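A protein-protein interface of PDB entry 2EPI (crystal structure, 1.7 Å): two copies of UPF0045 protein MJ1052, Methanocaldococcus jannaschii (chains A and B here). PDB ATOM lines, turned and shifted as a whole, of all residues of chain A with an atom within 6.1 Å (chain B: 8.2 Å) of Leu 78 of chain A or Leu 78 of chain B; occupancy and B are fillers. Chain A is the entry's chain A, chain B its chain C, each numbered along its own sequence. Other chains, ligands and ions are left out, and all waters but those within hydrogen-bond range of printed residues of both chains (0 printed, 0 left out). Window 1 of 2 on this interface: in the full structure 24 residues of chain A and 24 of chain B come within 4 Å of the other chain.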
ATOM      1  N   ALA A   9      18.929  -7.980 -27.438  1.00  0.00           N
ATOM      2  CA  ALA A   9      20.313  -7.634 -27.137  1.00  0.00           C
ATOM      3  C   ALA A   9      20.711  -8.079 -25.745  1.00  0.00           C
ATOM      4  O   ALA A   9      19.867  -8.464 -24.942  1.00  0.00           O
ATOM      5  CB  ALA A   9      20.493  -6.135 -27.259  1.00  0.00           C
ATOM      6  N   GLU A  10      22.010  -8.049 -25.474  1.00  0.00           N
ATOM      7  CA  GLU A  10      22.495  -8.397 -24.148  1.00  0.00           C
ATOM      8  C   GLU A  10      23.527  -7.363 -23.747  1.00  0.00           C
ATOM      9  O   GLU A  10      24.396  -6.992 -24.539  1.00  0.00           O
ATOM     10  CB  GLU A  10      23.109  -9.796 -24.112  1.00  0.00           C
ATOM     11  CG  GLU A  10      23.545 -10.195 -22.698  1.00  0.00           C
ATOM     12  CD  GLU A  10      23.941 -11.653 -22.583  1.00  0.00           C
ATOM     13  OE1 GLU A  10      24.705 -12.127 -23.447  1.00  0.00           O
ATOM     14  OE2 GLU A  10      23.490 -12.322 -21.619  1.00  0.00           O
ATOM     15  N   VAL A  11      23.420  -6.891 -22.514  1.00  0.00           N
ATOM     16  CA  VAL A  11      24.334  -5.880 -22.011  1.00  0.00           C
ATOM     17  C   VAL A  11      24.992  -6.333 -20.719  1.00  0.00           C
ATOM     18  O   VAL A  11      24.358  -6.959 -19.873  1.00  0.00           O
ATOM     19  CB  VAL A  11      23.592  -4.561 -21.718  1.00  0.00           C
ATOM     20  CG1 VAL A  11      24.537  -3.567 -21.037  1.00  0.00           C
ATOM     21  CG2 VAL A  11      23.025  -3.973 -23.011  1.00  0.00           C
ATOM     22  N   SER A  12      26.275  -6.030 -20.583  1.00  0.00           N
ATOM     23  CA  SER A  12      26.989  -6.346 -19.358  1.00  0.00           C
ATOM     24  C   SER A  12      27.893  -5.152 -19.107  1.00  0.00           C
ATOM     25  O   SER A  12      28.497  -4.606 -20.034  1.00  0.00           O
ATOM     26  CB  SER A  12      27.815  -7.626 -19.492  1.00  0.00           C
ATOM     27  OG  SER A  12      28.902  -7.458 -20.380  1.00  0.00           O
ATOM     28  N   LEU A  49      17.798  -7.598 -23.396  1.00  0.00           N
ATOM     29  CA  LEU A  49      16.802  -6.565 -23.639  1.00  0.00           C
ATOM     30  C   LEU A  49      16.123  -6.820 -24.971  1.00  0.00           C
ATOM     31  O   LEU A  49      16.724  -7.381 -25.889  1.00  0.00           O
ATOM     32  CB  LEU A  49      17.470  -5.181 -23.667  1.00  0.00           C
ATOM     33  CG  LEU A  49      18.347  -4.787 -22.477  1.00  0.00           C
ATOM     34  CD1 LEU A  49      19.171  -3.546 -22.823  1.00  0.00           C
ATOM     35  CD2 LEU A  49      17.469  -4.542 -21.256  1.00  0.00           C
ATOM     36  N   ILE A  56      17.525   0.938 -27.196  1.00  0.00           N
ATOM     37  CA  ILE A  56      18.516   0.084 -26.547  1.00  0.00           C
ATOM     38  C   ILE A  56      19.875   0.773 -26.536  1.00  0.00           C
ATOM     39  O   ILE A  56      20.613   0.684 -25.555  1.00  0.00           O
ATOM     40  CB  ILE A  56      18.610  -1.294 -27.249  1.00  0.00           C
ATOM     41  CG1 ILE A  56      17.391  -2.139 -26.856  1.00  0.00           C
ATOM     42  CG2 ILE A  56      19.910  -2.011 -26.859  1.00  0.00           C
ATOM     43  CD1 ILE A  56      17.319  -3.491 -27.535  1.00  0.00           C
ATOM     44  N   LEU A  57      20.201   1.469 -27.621  1.00  0.00           N
ATOM     45  CA  LEU A  57      21.473   2.183 -27.699  1.00  0.00           C
ATOM     46  C   LEU A  57      21.513   3.298 -26.655  1.00  0.00           C
ATOM     47  O   LEU A  57      22.527   3.495 -25.985  1.00  0.00           O
ATOM     48  CB  LEU A  57      21.671   2.760 -29.105  1.00  0.00           C
ATOM     49  CG  LEU A  57      21.944   1.702 -30.175  1.00  0.00           C
ATOM     50  CD1 LEU A  57      21.813   2.316 -31.558  1.00  0.00           C
ATOM     51  CD2 LEU A  57      23.328   1.116 -29.969  1.00  0.00           C
ATOM     52  N   PHE A  60      21.743   1.728 -23.263  1.00  0.00           N
ATOM     53  CA  PHE A  60      23.089   1.211 -23.079  1.00  0.00           C
ATOM     54  C   PHE A  60      24.011   2.347 -22.650  1.00  0.00           C
ATOM     55  O   PHE A  60      24.748   2.230 -21.670  1.00  0.00           O
ATOM     56  CB  PHE A  60      23.596   0.600 -24.386  1.00  0.00           C
ATOM     57  CG  PHE A  60      25.040   0.193 -24.346  1.00  0.00           C
ATOM     58  CD1 PHE A  60      25.472  -0.818 -23.494  1.00  0.00           C
ATOM     59  CD2 PHE A  60      25.970   0.810 -25.180  1.00  0.00           C
ATOM     60  CE1 PHE A  60      26.803  -1.216 -23.468  1.00  0.00           C
ATOM     61  CE2 PHE A  60      27.313   0.415 -25.161  1.00  0.00           C
ATOM     62  CZ  PHE A  60      27.726  -0.600 -24.304  1.00  0.00           C
ATOM     63  N   SER A  76      31.969  -1.699 -20.805  1.00  0.00           N
ATOM     64  CA  SER A  76      30.588  -2.110 -21.072  1.00  0.00           C
ATOM     65  C   SER A  76      30.432  -2.807 -22.413  1.00  0.00           C
ATOM     66  O   SER A  76      31.033  -2.397 -23.411  1.00  0.00           O
ATOM     67  CB  SER A  76      29.671  -0.889 -21.005  1.00  0.00           C
ATOM     68  OG  SER A  76      29.724  -0.305 -19.716  1.00  0.00           O
ATOM     69  N   SER A  77      29.613  -3.856 -22.437  1.00  0.00           N
ATOM     70  CA  SER A  77      29.405  -4.630 -23.654  1.00  0.00           C
ATOM     71  C   SER A  77      27.945  -4.652 -24.096  1.00  0.00           C
ATOM     72  O   SER A  77      27.043  -4.845 -23.276  1.00  0.00           O
ATOM     73  CB  SER A  77      29.882  -6.078 -23.441  1.00  0.00           C
ATOM     74  OG  SER A  77      31.248  -6.135 -23.037  1.00  0.00           O
ATOM     75  N   LEU A  78      27.724  -4.450 -25.394  1.00  0.00           N
ATOM     76  CA  LEU A  78      26.393  -4.477 -25.985  1.00  0.00           C
ATOM     77  C   LEU A  78      26.427  -5.430 -27.173  1.00  0.00           C
ATOM     78  O   LEU A  78      27.293  -5.319 -28.041  1.00  0.00           O
ATOM     79  CB  LEU A  78      25.977  -3.081 -26.479  1.00  0.00           C
ATOM     80  CG  LEU A  78      24.706  -3.000 -27.347  1.00  0.00           C
ATOM     81  CD1 LEU A  78      23.482  -3.441 -26.545  1.00  0.00           C
ATOM     82  CD2 LEU A  78      24.518  -1.569 -27.850  1.00  0.00           C
ATOM     83  N   LYS A  79      25.509  -6.387 -27.199  1.00  0.00           N
ATOM     84  CA  LYS A  79      25.450  -7.315 -28.319  1.00  0.00           C
ATOM     85  C   LYS A  79      24.048  -7.229 -28.890  1.00  0.00           C
ATOM     86  O   LYS A  79      23.073  -7.320 -28.150  1.00  0.00           O
ATOM     87  CB  LYS A  79      25.744  -8.742 -27.859  1.00  0.00           C
ATOM     88  CG  LYS A  79      25.738  -9.745 -28.999  1.00  0.00           C
ATOM     89  CD  LYS A  79      26.141 -11.132 -28.525  1.00  0.00           C
ATOM     90  CE  LYS A  79      27.593 -11.179 -28.087  1.00  0.00           C
ATOM     91  NZ  LYS A  79      27.931 -12.513 -27.505  1.00  0.00           N
ATOM     92  N   ILE A  80      23.954  -7.033 -30.201  1.00  0.00           N
ATOM     93  CA  ILE A  80      22.665  -6.924 -30.873  1.00  0.00           C
ATOM     94  C   ILE A  80      22.455  -8.104 -31.802  1.00  0.00           C
ATOM     95  O   ILE A  80      23.365  -8.495 -32.528  1.00  0.00           O
ATOM     96  CB  ILE A  80      22.579  -5.639 -31.734  1.00  0.00           C
ATOM     97  CG1 ILE A  80      22.781  -4.402 -30.858  1.00  0.00           C
ATOM     98  CG2 ILE A  80      21.235  -5.583 -32.447  1.00  0.00           C
ATOM     99  CD1 ILE A  80      21.813  -4.287 -29.717  1.00  0.00           C
ATOM    100  N   VAL B   7      36.333   7.702 -26.053  1.00  0.00           N
ATOM    101  CA  VAL B   7      36.364   6.374 -25.454  1.00  0.00           C
ATOM    102  C   VAL B   7      37.059   5.465 -26.458  1.00  0.00           C
ATOM    103  O   VAL B   7      37.251   5.840 -27.617  1.00  0.00           O
ATOM    104  CB  VAL B   7      34.936   5.811 -25.197  1.00  0.00           C
ATOM    105  CG1 VAL B   7      34.120   6.802 -24.385  1.00  0.00           C
ATOM    106  CG2 VAL B   7      34.244   5.498 -26.518  1.00  0.00           C
ATOM    107  N   VAL B   8      37.460   4.282 -26.009  1.00  0.00           N
ATOM    108  CA  VAL B   8      38.089   3.319 -26.895  1.00  0.00           C
ATOM    109  C   VAL B   8      37.104   2.167 -26.946  1.00  0.00           C
ATOM    110  O   VAL B   8      36.506   1.825 -25.929  1.00  0.00           O
ATOM    111  CB  VAL B   8      39.427   2.817 -26.343  1.00  0.00           C
ATOM    112  CG1 VAL B   8      40.033   1.805 -27.305  1.00  0.00           C
ATOM    113  CG2 VAL B   8      40.369   3.994 -26.136  1.00  0.00           C
ATOM    114  N   ALA B   9      36.927   1.572 -28.118  1.00  0.00           N
ATOM    115  CA  ALA B   9      35.973   0.481 -28.244  1.00  0.00           C
ATOM    116  C   ALA B   9      36.414  -0.597 -29.215  1.00  0.00           C
ATOM    117  O   ALA B   9      37.384  -0.431 -29.952  1.00  0.00           O
ATOM    118  CB  ALA B   9      34.630   1.043 -28.691  1.00  0.00           C
ATOM    119  N   GLU B  10      35.713  -1.726 -29.186  1.00  0.00           N
ATOM    120  CA  GLU B  10      35.986  -2.801 -30.126  1.00  0.00           C
ATOM    121  C   GLU B  10      34.648  -3.291 -30.648  1.00  0.00           C
ATOM    122  O   GLU B  10      33.707  -3.512 -29.882  1.00  0.00           O
ATOM    123  CB  GLU B  10      36.758  -3.956 -29.494  1.00  0.00           C
ATOM    124  CG  GLU B  10      36.991  -5.070 -30.501  1.00  0.00           C
ATOM    125  CD  GLU B  10      37.962  -6.120 -30.018  1.00  0.00           C
ATOM    126  OE1 GLU B  10      37.792  -6.605 -28.879  1.00  0.00           O
ATOM    127  OE2 GLU B  10      38.891  -6.464 -30.786  1.00  0.00           O
ATOM    128  N   VAL B  11      34.564  -3.455 -31.961  1.00  0.00           N
ATOM    129  CA  VAL B  11      33.324  -3.871 -32.598  1.00  0.00           C
ATOM    130  C   VAL B  11      33.522  -5.049 -33.539  1.00  0.00           C
ATOM    131  O   VAL B  11      34.598  -5.228 -34.104  1.00  0.00           O
ATOM    132  CB  VAL B  11      32.730  -2.697 -33.422  1.00  0.00           C
ATOM    133  CG1 VAL B  11      31.481  -3.139 -34.146  1.00  0.00           C
ATOM    134  CG2 VAL B  11      32.422  -1.521 -32.513  1.00  0.00           C
ATOM    135  N   SER B  12      32.474  -5.852 -33.689  1.00  0.00           N
ATOM    136  CA  SER B  12      32.474  -6.986 -34.606  1.00  0.00           C
ATOM    137  C   SER B  12      31.050  -7.098 -35.148  1.00  0.00           C
ATOM    138  O   SER B  12      30.084  -7.070 -34.382  1.00  0.00           O
ATOM    139  CB  SER B  12      32.881  -8.283 -33.894  1.00  0.00           C
ATOM    140  OG  SER B  12      31.913  -8.679 -32.942  1.00  0.00           O
ATOM    141  N   ILE B  13      30.923  -7.172 -36.472  1.00  0.00           N
ATOM    142  CA  ILE B  13      29.621  -7.291 -37.130  1.00  0.00           C
ATOM    143  C   ILE B  13      29.636  -8.618 -37.877  1.00  0.00           C
ATOM    144  O   ILE B  13      30.309  -8.759 -38.899  1.00  0.00           O
ATOM    145  CB  ILE B  13      29.373  -6.144 -38.149  1.00  0.00           C
ATOM    146  CG1 ILE B  13      29.316  -4.794 -37.433  1.00  0.00           C
ATOM    147  CG2 ILE B  13      28.071  -6.380 -38.895  1.00  0.00           C
ATOM    148  CD1 ILE B  13      30.658  -4.279 -36.998  1.00  0.00           C
ATOM    149  N   PHE B  33      32.874   2.823 -40.601  1.00  0.00           N
ATOM    150  CA  PHE B  33      33.551   3.439 -39.464  1.00  0.00           C
ATOM    151  C   PHE B  33      34.450   4.586 -39.909  1.00  0.00           C
ATOM    152  O   PHE B  33      34.456   5.658 -39.301  1.00  0.00           O
ATOM    153  CB  PHE B  33      34.409   2.413 -38.713  1.00  0.00           C
ATOM    154  CG  PHE B  33      33.637   1.239 -38.185  1.00  0.00           C
ATOM    155  CD1 PHE B  33      32.521   1.428 -37.377  1.00  0.00           C
ATOM    156  CD2 PHE B  33      34.029  -0.060 -38.495  1.00  0.00           C
ATOM    157  CE1 PHE B  33      31.804   0.338 -36.884  1.00  0.00           C
ATOM    158  CE2 PHE B  33      33.320  -1.157 -38.007  1.00  0.00           C
ATOM    159  CZ  PHE B  33      32.206  -0.955 -37.202  1.00  0.00           C
ATOM    160  N   THR B  47      37.263  -4.779 -34.846  1.00  0.00           N
ATOM    161  CA  THR B  47      37.825  -3.461 -35.104  1.00  0.00           C
ATOM    162  C   THR B  47      37.815  -2.576 -33.866  1.00  0.00           C
ATOM    163  O   THR B  47      36.777  -2.407 -33.221  1.00  0.00           O
ATOM    164  CB  THR B  47      37.048  -2.756 -36.232  1.00  0.00           C
ATOM    165  OG1 THR B  47      37.224  -3.482 -37.454  1.00  0.00           O
ATOM    166  CG2 THR B  47      37.536  -1.331 -36.413  1.00  0.00           C
ATOM    167  N   LEU B  49      38.108   1.054 -32.089  1.00  0.00           N
ATOM    168  CA  LEU B  49      37.783   2.429 -32.444  1.00  0.00           C
ATOM    169  C   LEU B  49      38.124   3.393 -31.321  1.00  0.00           C
ATOM    170  O   LEU B  49      38.073   3.041 -30.141  1.00  0.00           O
ATOM    171  CB  LEU B  49      36.287   2.551 -32.751  1.00  0.00           C
ATOM    172  CG  LEU B  49      35.696   1.585 -33.780  1.00  0.00           C
ATOM    173  CD1 LEU B  49      34.175   1.726 -33.794  1.00  0.00           C
ATOM    174  CD2 LEU B  49      36.280   1.872 -35.155  1.00  0.00           C
ATOM    175  N   LEU B  53      31.934   9.030 -27.963  1.00  0.00           N
ATOM    176  CA  LEU B  53      31.023   7.928 -27.668  1.00  0.00           C
ATOM    177  C   LEU B  53      29.795   7.947 -28.571  1.00  0.00           C
ATOM    178  O   LEU B  53      29.430   6.918 -29.144  1.00  0.00           O
ATOM    179  CB  LEU B  53      30.590   7.977 -26.199  1.00  0.00           C
ATOM    180  CG  LEU B  53      29.615   6.895 -25.713  1.00  0.00           C
ATOM    181  CD1 LEU B  53      30.158   5.510 -26.021  1.00  0.00           C
ATOM    182  CD2 LEU B  53      29.406   7.059 -24.213  1.00  0.00           C
ATOM    183  N   ILE B  56      30.620   6.827 -32.041  1.00  0.00           N
ATOM    184  CA  ILE B  56      30.875   5.393 -32.107  1.00  0.00           C
ATOM    185  C   ILE B  56      29.555   4.625 -32.122  1.00  0.00           C
ATOM    186  O   ILE B  56      29.411   3.644 -32.851  1.00  0.00           O
ATOM    187  CB  ILE B  56      31.763   4.940 -30.919  1.00  0.00           C
ATOM    188  CG1 ILE B  56      33.200   5.426 -31.152  1.00  0.00           C
ATOM    189  CG2 ILE B  56      31.724   3.418 -30.767  1.00  0.00           C
ATOM    190  CD1 ILE B  56      34.170   5.093 -30.039  1.00  0.00           C
ATOM    191  N   LEU B  57      28.588   5.079 -31.333  1.00  0.00           N
ATOM    192  CA  LEU B  57      27.284   4.430 -31.301  1.00  0.00           C
ATOM    193  C   LEU B  57      26.625   4.572 -32.671  1.00  0.00           C
ATOM    194  O   LEU B  57      26.079   3.607 -33.218  1.00  0.00           O
ATOM    195  CB  LEU B  57      26.410   5.063 -30.220  1.00  0.00           C
ATOM    196  CG  LEU B  57      26.829   4.734 -28.784  1.00  0.00           C
ATOM    197  CD1 LEU B  57      26.044   5.585 -27.808  1.00  0.00           C
ATOM    198  CD2 LEU B  57      26.601   3.242 -28.512  1.00  0.00           C
ATOM    199  N   LYS B  58      26.693   5.776 -33.235  1.00  0.00           N
ATOM    200  CA  LYS B  58      26.109   6.027 -34.548  1.00  0.00           C
ATOM    201  C   LYS B  58      26.775   5.136 -35.588  1.00  0.00           C
ATOM    202  O   LYS B  58      26.102   4.499 -36.401  1.00  0.00           O
ATOM    203  CB  LYS B  58      26.292   7.497 -34.947  1.00  0.00           C
ATOM    204  CG  LYS B  58      25.643   8.495 -34.005  1.00  0.00           C
ATOM    205  CD  LYS B  58      25.968   9.924 -34.423  1.00  0.00           C
ATOM    206  CE  LYS B  58      25.390  10.939 -33.446  1.00  0.00           C
ATOM    207  NZ  LYS B  58      25.720  12.336 -33.847  1.00  0.00           N
ATOM    208  N   ALA B  59      28.102   5.097 -35.561  1.00  0.00           N
ATOM    209  CA  ALA B  59      28.864   4.289 -36.502  1.00  0.00           C
ATOM    210  C   ALA B  59      28.518   2.814 -36.349  1.00  0.00           C
ATOM    211  O   ALA B  59      28.361   2.090 -37.336  1.00  0.00           O
ATOM    212  CB  ALA B  59      30.353   4.501 -36.285  1.00  0.00           C
ATOM    213  N   PHE B  60      28.402   2.378 -35.098  1.00  0.00           N
ATOM    214  CA  PHE B  60      28.072   0.991 -34.794  1.00  0.00           C
ATOM    215  C   PHE B  60      26.734   0.628 -35.431  1.00  0.00           C
ATOM    216  O   PHE B  60      26.613  -0.400 -36.097  1.00  0.00           O
ATOM    217  CB  PHE B  60      28.000   0.802 -33.273  1.00  0.00           C
ATOM    218  CG  PHE B  60      27.571  -0.577 -32.844  1.00  0.00           C
ATOM    219  CD1 PHE B  60      28.351  -1.688 -33.143  1.00  0.00           C
ATOM    220  CD2 PHE B  60      26.385  -0.759 -32.135  1.00  0.00           C
ATOM    221  CE1 PHE B  60      27.955  -2.971 -32.743  1.00  0.00           C
ATOM    222  CE2 PHE B  60      25.976  -2.036 -31.730  1.00  0.00           C
ATOM    223  CZ  PHE B  60      26.762  -3.142 -32.033  1.00  0.00           C
ATOM    224  N   LYS B  61      25.733   1.477 -35.234  1.00  0.00           N
ATOM    225  CA  LYS B  61      24.417   1.206 -35.792  1.00  0.00           C
ATOM    226  C   LYS B  61      24.459   1.147 -37.316  1.00  0.00           C
ATOM    227  O   LYS B  61      23.890   0.238 -37.921  1.00  0.00           O
ATOM    228  CB  LYS B  61      23.408   2.267 -35.357  1.00  0.00           C
ATOM    229  CG  LYS B  61      22.008   2.013 -35.909  1.00  0.00           C
ATOM    230  CD  LYS B  61      21.080   3.179 -35.636  1.00  0.00           C
ATOM    231  CE  LYS B  61      19.716   2.952 -36.273  1.00  0.00           C
ATOM    232  NZ  LYS B  61      18.825   4.133 -36.085  1.00  0.00           N
ATOM    233  N   VAL B  75      24.594 -10.377 -36.067  1.00  0.00           N
ATOM    234  CA  VAL B  75      24.867 -10.316 -34.631  1.00  0.00           C
ATOM    235  C   VAL B  75      26.075  -9.399 -34.498  1.00  0.00           C
ATOM    236  O   VAL B  75      27.183  -9.747 -34.913  1.00  0.00           O
ATOM    237  CB  VAL B  75      25.209 -11.699 -34.041  1.00  0.00           C
ATOM    238  CG1 VAL B  75      25.554 -11.557 -32.557  1.00  0.00           C
ATOM    239  CG2 VAL B  75      24.033 -12.642 -34.211  1.00  0.00           C
ATOM    240  N   SER B  76      25.853  -8.217 -33.936  1.00  0.00           N
ATOM    241  CA  SER B  76      26.921  -7.243 -33.780  1.00  0.00           C
ATOM    242  C   SER B  76      27.247  -6.997 -32.320  1.00  0.00           C
ATOM    243  O   SER B  76      26.358  -6.985 -31.472  1.00  0.00           O
ATOM    244  CB  SER B  76      26.517  -5.934 -34.448  1.00  0.00           C
ATOM    245  OG  SER B  76      26.140  -6.182 -35.794  1.00  0.00           O
ATOM    246  N   SER B  77      28.530  -6.794 -32.047  1.00  0.00           N
ATOM    247  CA  SER B  77      29.008  -6.559 -30.688  1.00  0.00           C
ATOM    248  C   SER B  77      29.763  -5.239 -30.578  1.00  0.00           C
ATOM    249  O   SER B  77      30.561  -4.893 -31.450  1.00  0.00           O
ATOM    250  CB  SER B  77      29.940  -7.696 -30.261  1.00  0.00           C
ATOM    251  OG  SER B  77      29.296  -8.954 -30.346  1.00  0.00           O
ATOM    252  N   LEU B  78      29.506  -4.512 -29.497  1.00  0.00           N
ATOM    253  CA  LEU B  78      30.172  -3.242 -29.234  1.00  0.00           C
ATOM    254  C   LEU B  78      30.650  -3.272 -27.789  1.00  0.00           C
ATOM    255  O   LEU B  78      29.858  -3.497 -26.875  1.00  0.00           O
ATOM    256  CB  LEU B  78      29.207  -2.064 -29.427  1.00  0.00           C
ATOM    257  CG  LEU B  78      29.651  -0.688 -28.899  1.00  0.00           C
ATOM    258  CD1 LEU B  78      30.927  -0.245 -29.598  1.00  0.00           C
ATOM    259  CD2 LEU B  78      28.545   0.334 -29.110  1.00  0.00           C
ATOM    260  N   LYS B  79      31.946  -3.071 -27.588  1.00  0.00           N
ATOM    261  CA  LYS B  79      32.499  -3.053 -26.242  1.00  0.00           C
ATOM    262  C   LYS B  79      33.137  -1.687 -26.041  1.00  0.00           C
ATOM    263  O   LYS B  79      33.977  -1.268 -26.839  1.00  0.00           O
ATOM    264  CB  LYS B  79      33.540  -4.163 -26.076  1.00  0.00           C
ATOM    265  CG  LYS B  79      34.148  -4.237 -24.687  1.00  0.00           C
ATOM    266  CD  LYS B  79      35.164  -5.371 -24.584  1.00  0.00           C
ATOM    267  CE  LYS B  79      34.488  -6.727 -24.667  1.00  0.00           C
ATOM    268  NZ  LYS B  79      35.495  -7.836 -24.721  1.00  0.00           N
ATOM    269  N   ILE B  80      32.720  -0.993 -24.987  1.00  0.00           N
ATOM    270  CA  ILE B  80      33.235   0.333 -24.666  1.00  0.00           C
ATOM    271  C   ILE B  80      34.121   0.289 -23.425  1.00  0.00           C
ATOM    272  O   ILE B  80      33.757  -0.310 -22.419  1.00  0.00           O
ATOM    273  CB  ILE B  80      32.075   1.325 -24.390  1.00  0.00           C
ATOM    274  CG1 ILE B  80      31.193   1.452 -25.632  1.00  0.00           C
ATOM    275  CG2 ILE B  80      32.622   2.686 -23.977  1.00  0.00           C
ATOM    276  CD1 ILE B  80      31.909   1.996 -26.832  1.00  0.00           C
ATOM    277  N   ASP B  81      35.292   0.913 -23.509  1.00  0.00           N
ATOM    278  CA  ASP B  81      36.212   0.974 -22.376  1.00  0.00           C
ATOM    279  C   ASP B  81      36.445   2.468 -22.153  1.00  0.00           C
ATOM    280  O   ASP B  81      37.079   3.126 -22.976  1.00  0.00           O
ATOM    281  CB  ASP B  81      37.530   0.281 -22.726  1.00  0.00           C
ATOM    282  CG  ASP B  81      38.447   0.110 -21.526  1.00  0.00           C
ATOM    283  OD1 ASP B  81      38.306   0.869 -20.539  1.00  0.00           O
ATOM    284  OD2 ASP B  81      39.323  -0.780 -21.586  1.00  0.00           O
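The backbone carbonyl oxygen (O) of Ser 76 of chain A lies within hydrogen-bond range of the backbone NH (N) of Ile 80 of chain B (2.7 Å). N of Leu 78 of chain A sits at hydrogen-bond distance from O of Leu 78 of chain B, 2.8 Å away. The backbone carbonyl oxygen (O) of Ser 76 of chain B lies within hydrogen-bond range of the backbone NH (N) of Ile 80 of chain A (2.7 Å).
The backbone carbonyl oxygen (O) of Glu 10 of chain A is in hydrogen-bond range of the backbone NH (N) of Lys 79 of chain A (2.9 Å). N of Ser 77 of chain A is in hydrogen-bond range of O of Ser 12 of chain A (2.8 Å). The backbone NH of Lys 79 of chain B sits at hydrogen-bond distance from the backbone carbonyl oxygen of Glu 10 of chain B (2.9 Å). The backbone NH (N) of Ser 77 of chain B sits at hydrogen-bond distance from the backbone carbonyl oxygen (O) of Ser 12 of chain B (2.8 Å).
Ser 76 of chain A touches Leu 78 of chain B (O to O, 3.8 Å). O of Ser 76 of chain A touches CA of Lys 79 of chain B, 3.3 Å away. CA of Ser 77 of chain A touches O of Leu 78 of chain B, 3.4 Å away. CE of Lys 79 of chain B touches OG of Ser 77 of chain A (3.7 Å). Leu 78 of chain A touches Ser 76 of chain B (O to O, 3.9 Å). O of Leu 78 of chain A touches CA of Ser 77 of chain B, at 3.4 Å. CG of Lys 79 of chain A touches CG1 of Val 75 of chain B, 3.997 Å away. Lys 79 of chain A touches Ser 76 of chain B. Ser 77 of chain B touches Lys 79 of chain A (OG to CE, 3.6 Å). Ile 80 of chain A touches Val 75 of chain B.
Printed residues of chain B within 4 Å of Ile 80 of chain A: Val 75 (3.2 Å) and Ser 76 (2.7 Å). Val 11 of chain B touches none of the printed residues of chain A. Printed residues of chain A within 4 Å of Val 75 of chain B: Lys 79 and Ile 80. Printed residues of chain A within 4 Å of Ser 76 of chain B: Leu 78, Lys 79 and Ile 80. Leu 78 of chain B touches three residues of chain A. Of the printed residues of chain A, Lys 79 of chain B touches Ser 76 (3.3 Å) and Ser 77 (3.7 Å).
Of the 13 printed residues of chain A, 5 touch a printed residue of chain B. Among the printed residues, 13 pairs touch across the chains. Among the printed residues, no Asp or Glu carboxylate lies within 4 Å of a Lys or Arg side-chain nitrogen of the other chain.
Ser 76 of chain A touches Lys 79 of chain B, and with the chains exchanged Lys 79 of chain A touches Ser 76 of chain B. Ser 77 of chain A touches Leu 78 of chain B, and with the chains exchanged Leu 78 of chain A touches Ser 77 of chain B. Ser 77 of chain A touches Lys 79 of chain B, and with the chains exchanged Lys 79 of chain A touches Ser 77 of chain B. Leu 78 of chain A touches its own counterpart, Leu 78 of chain B. Positions printed for both chains: 9, 10, 11, 12, 49, 56, 57, 60, 76, 77, 78, 79 and 80.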
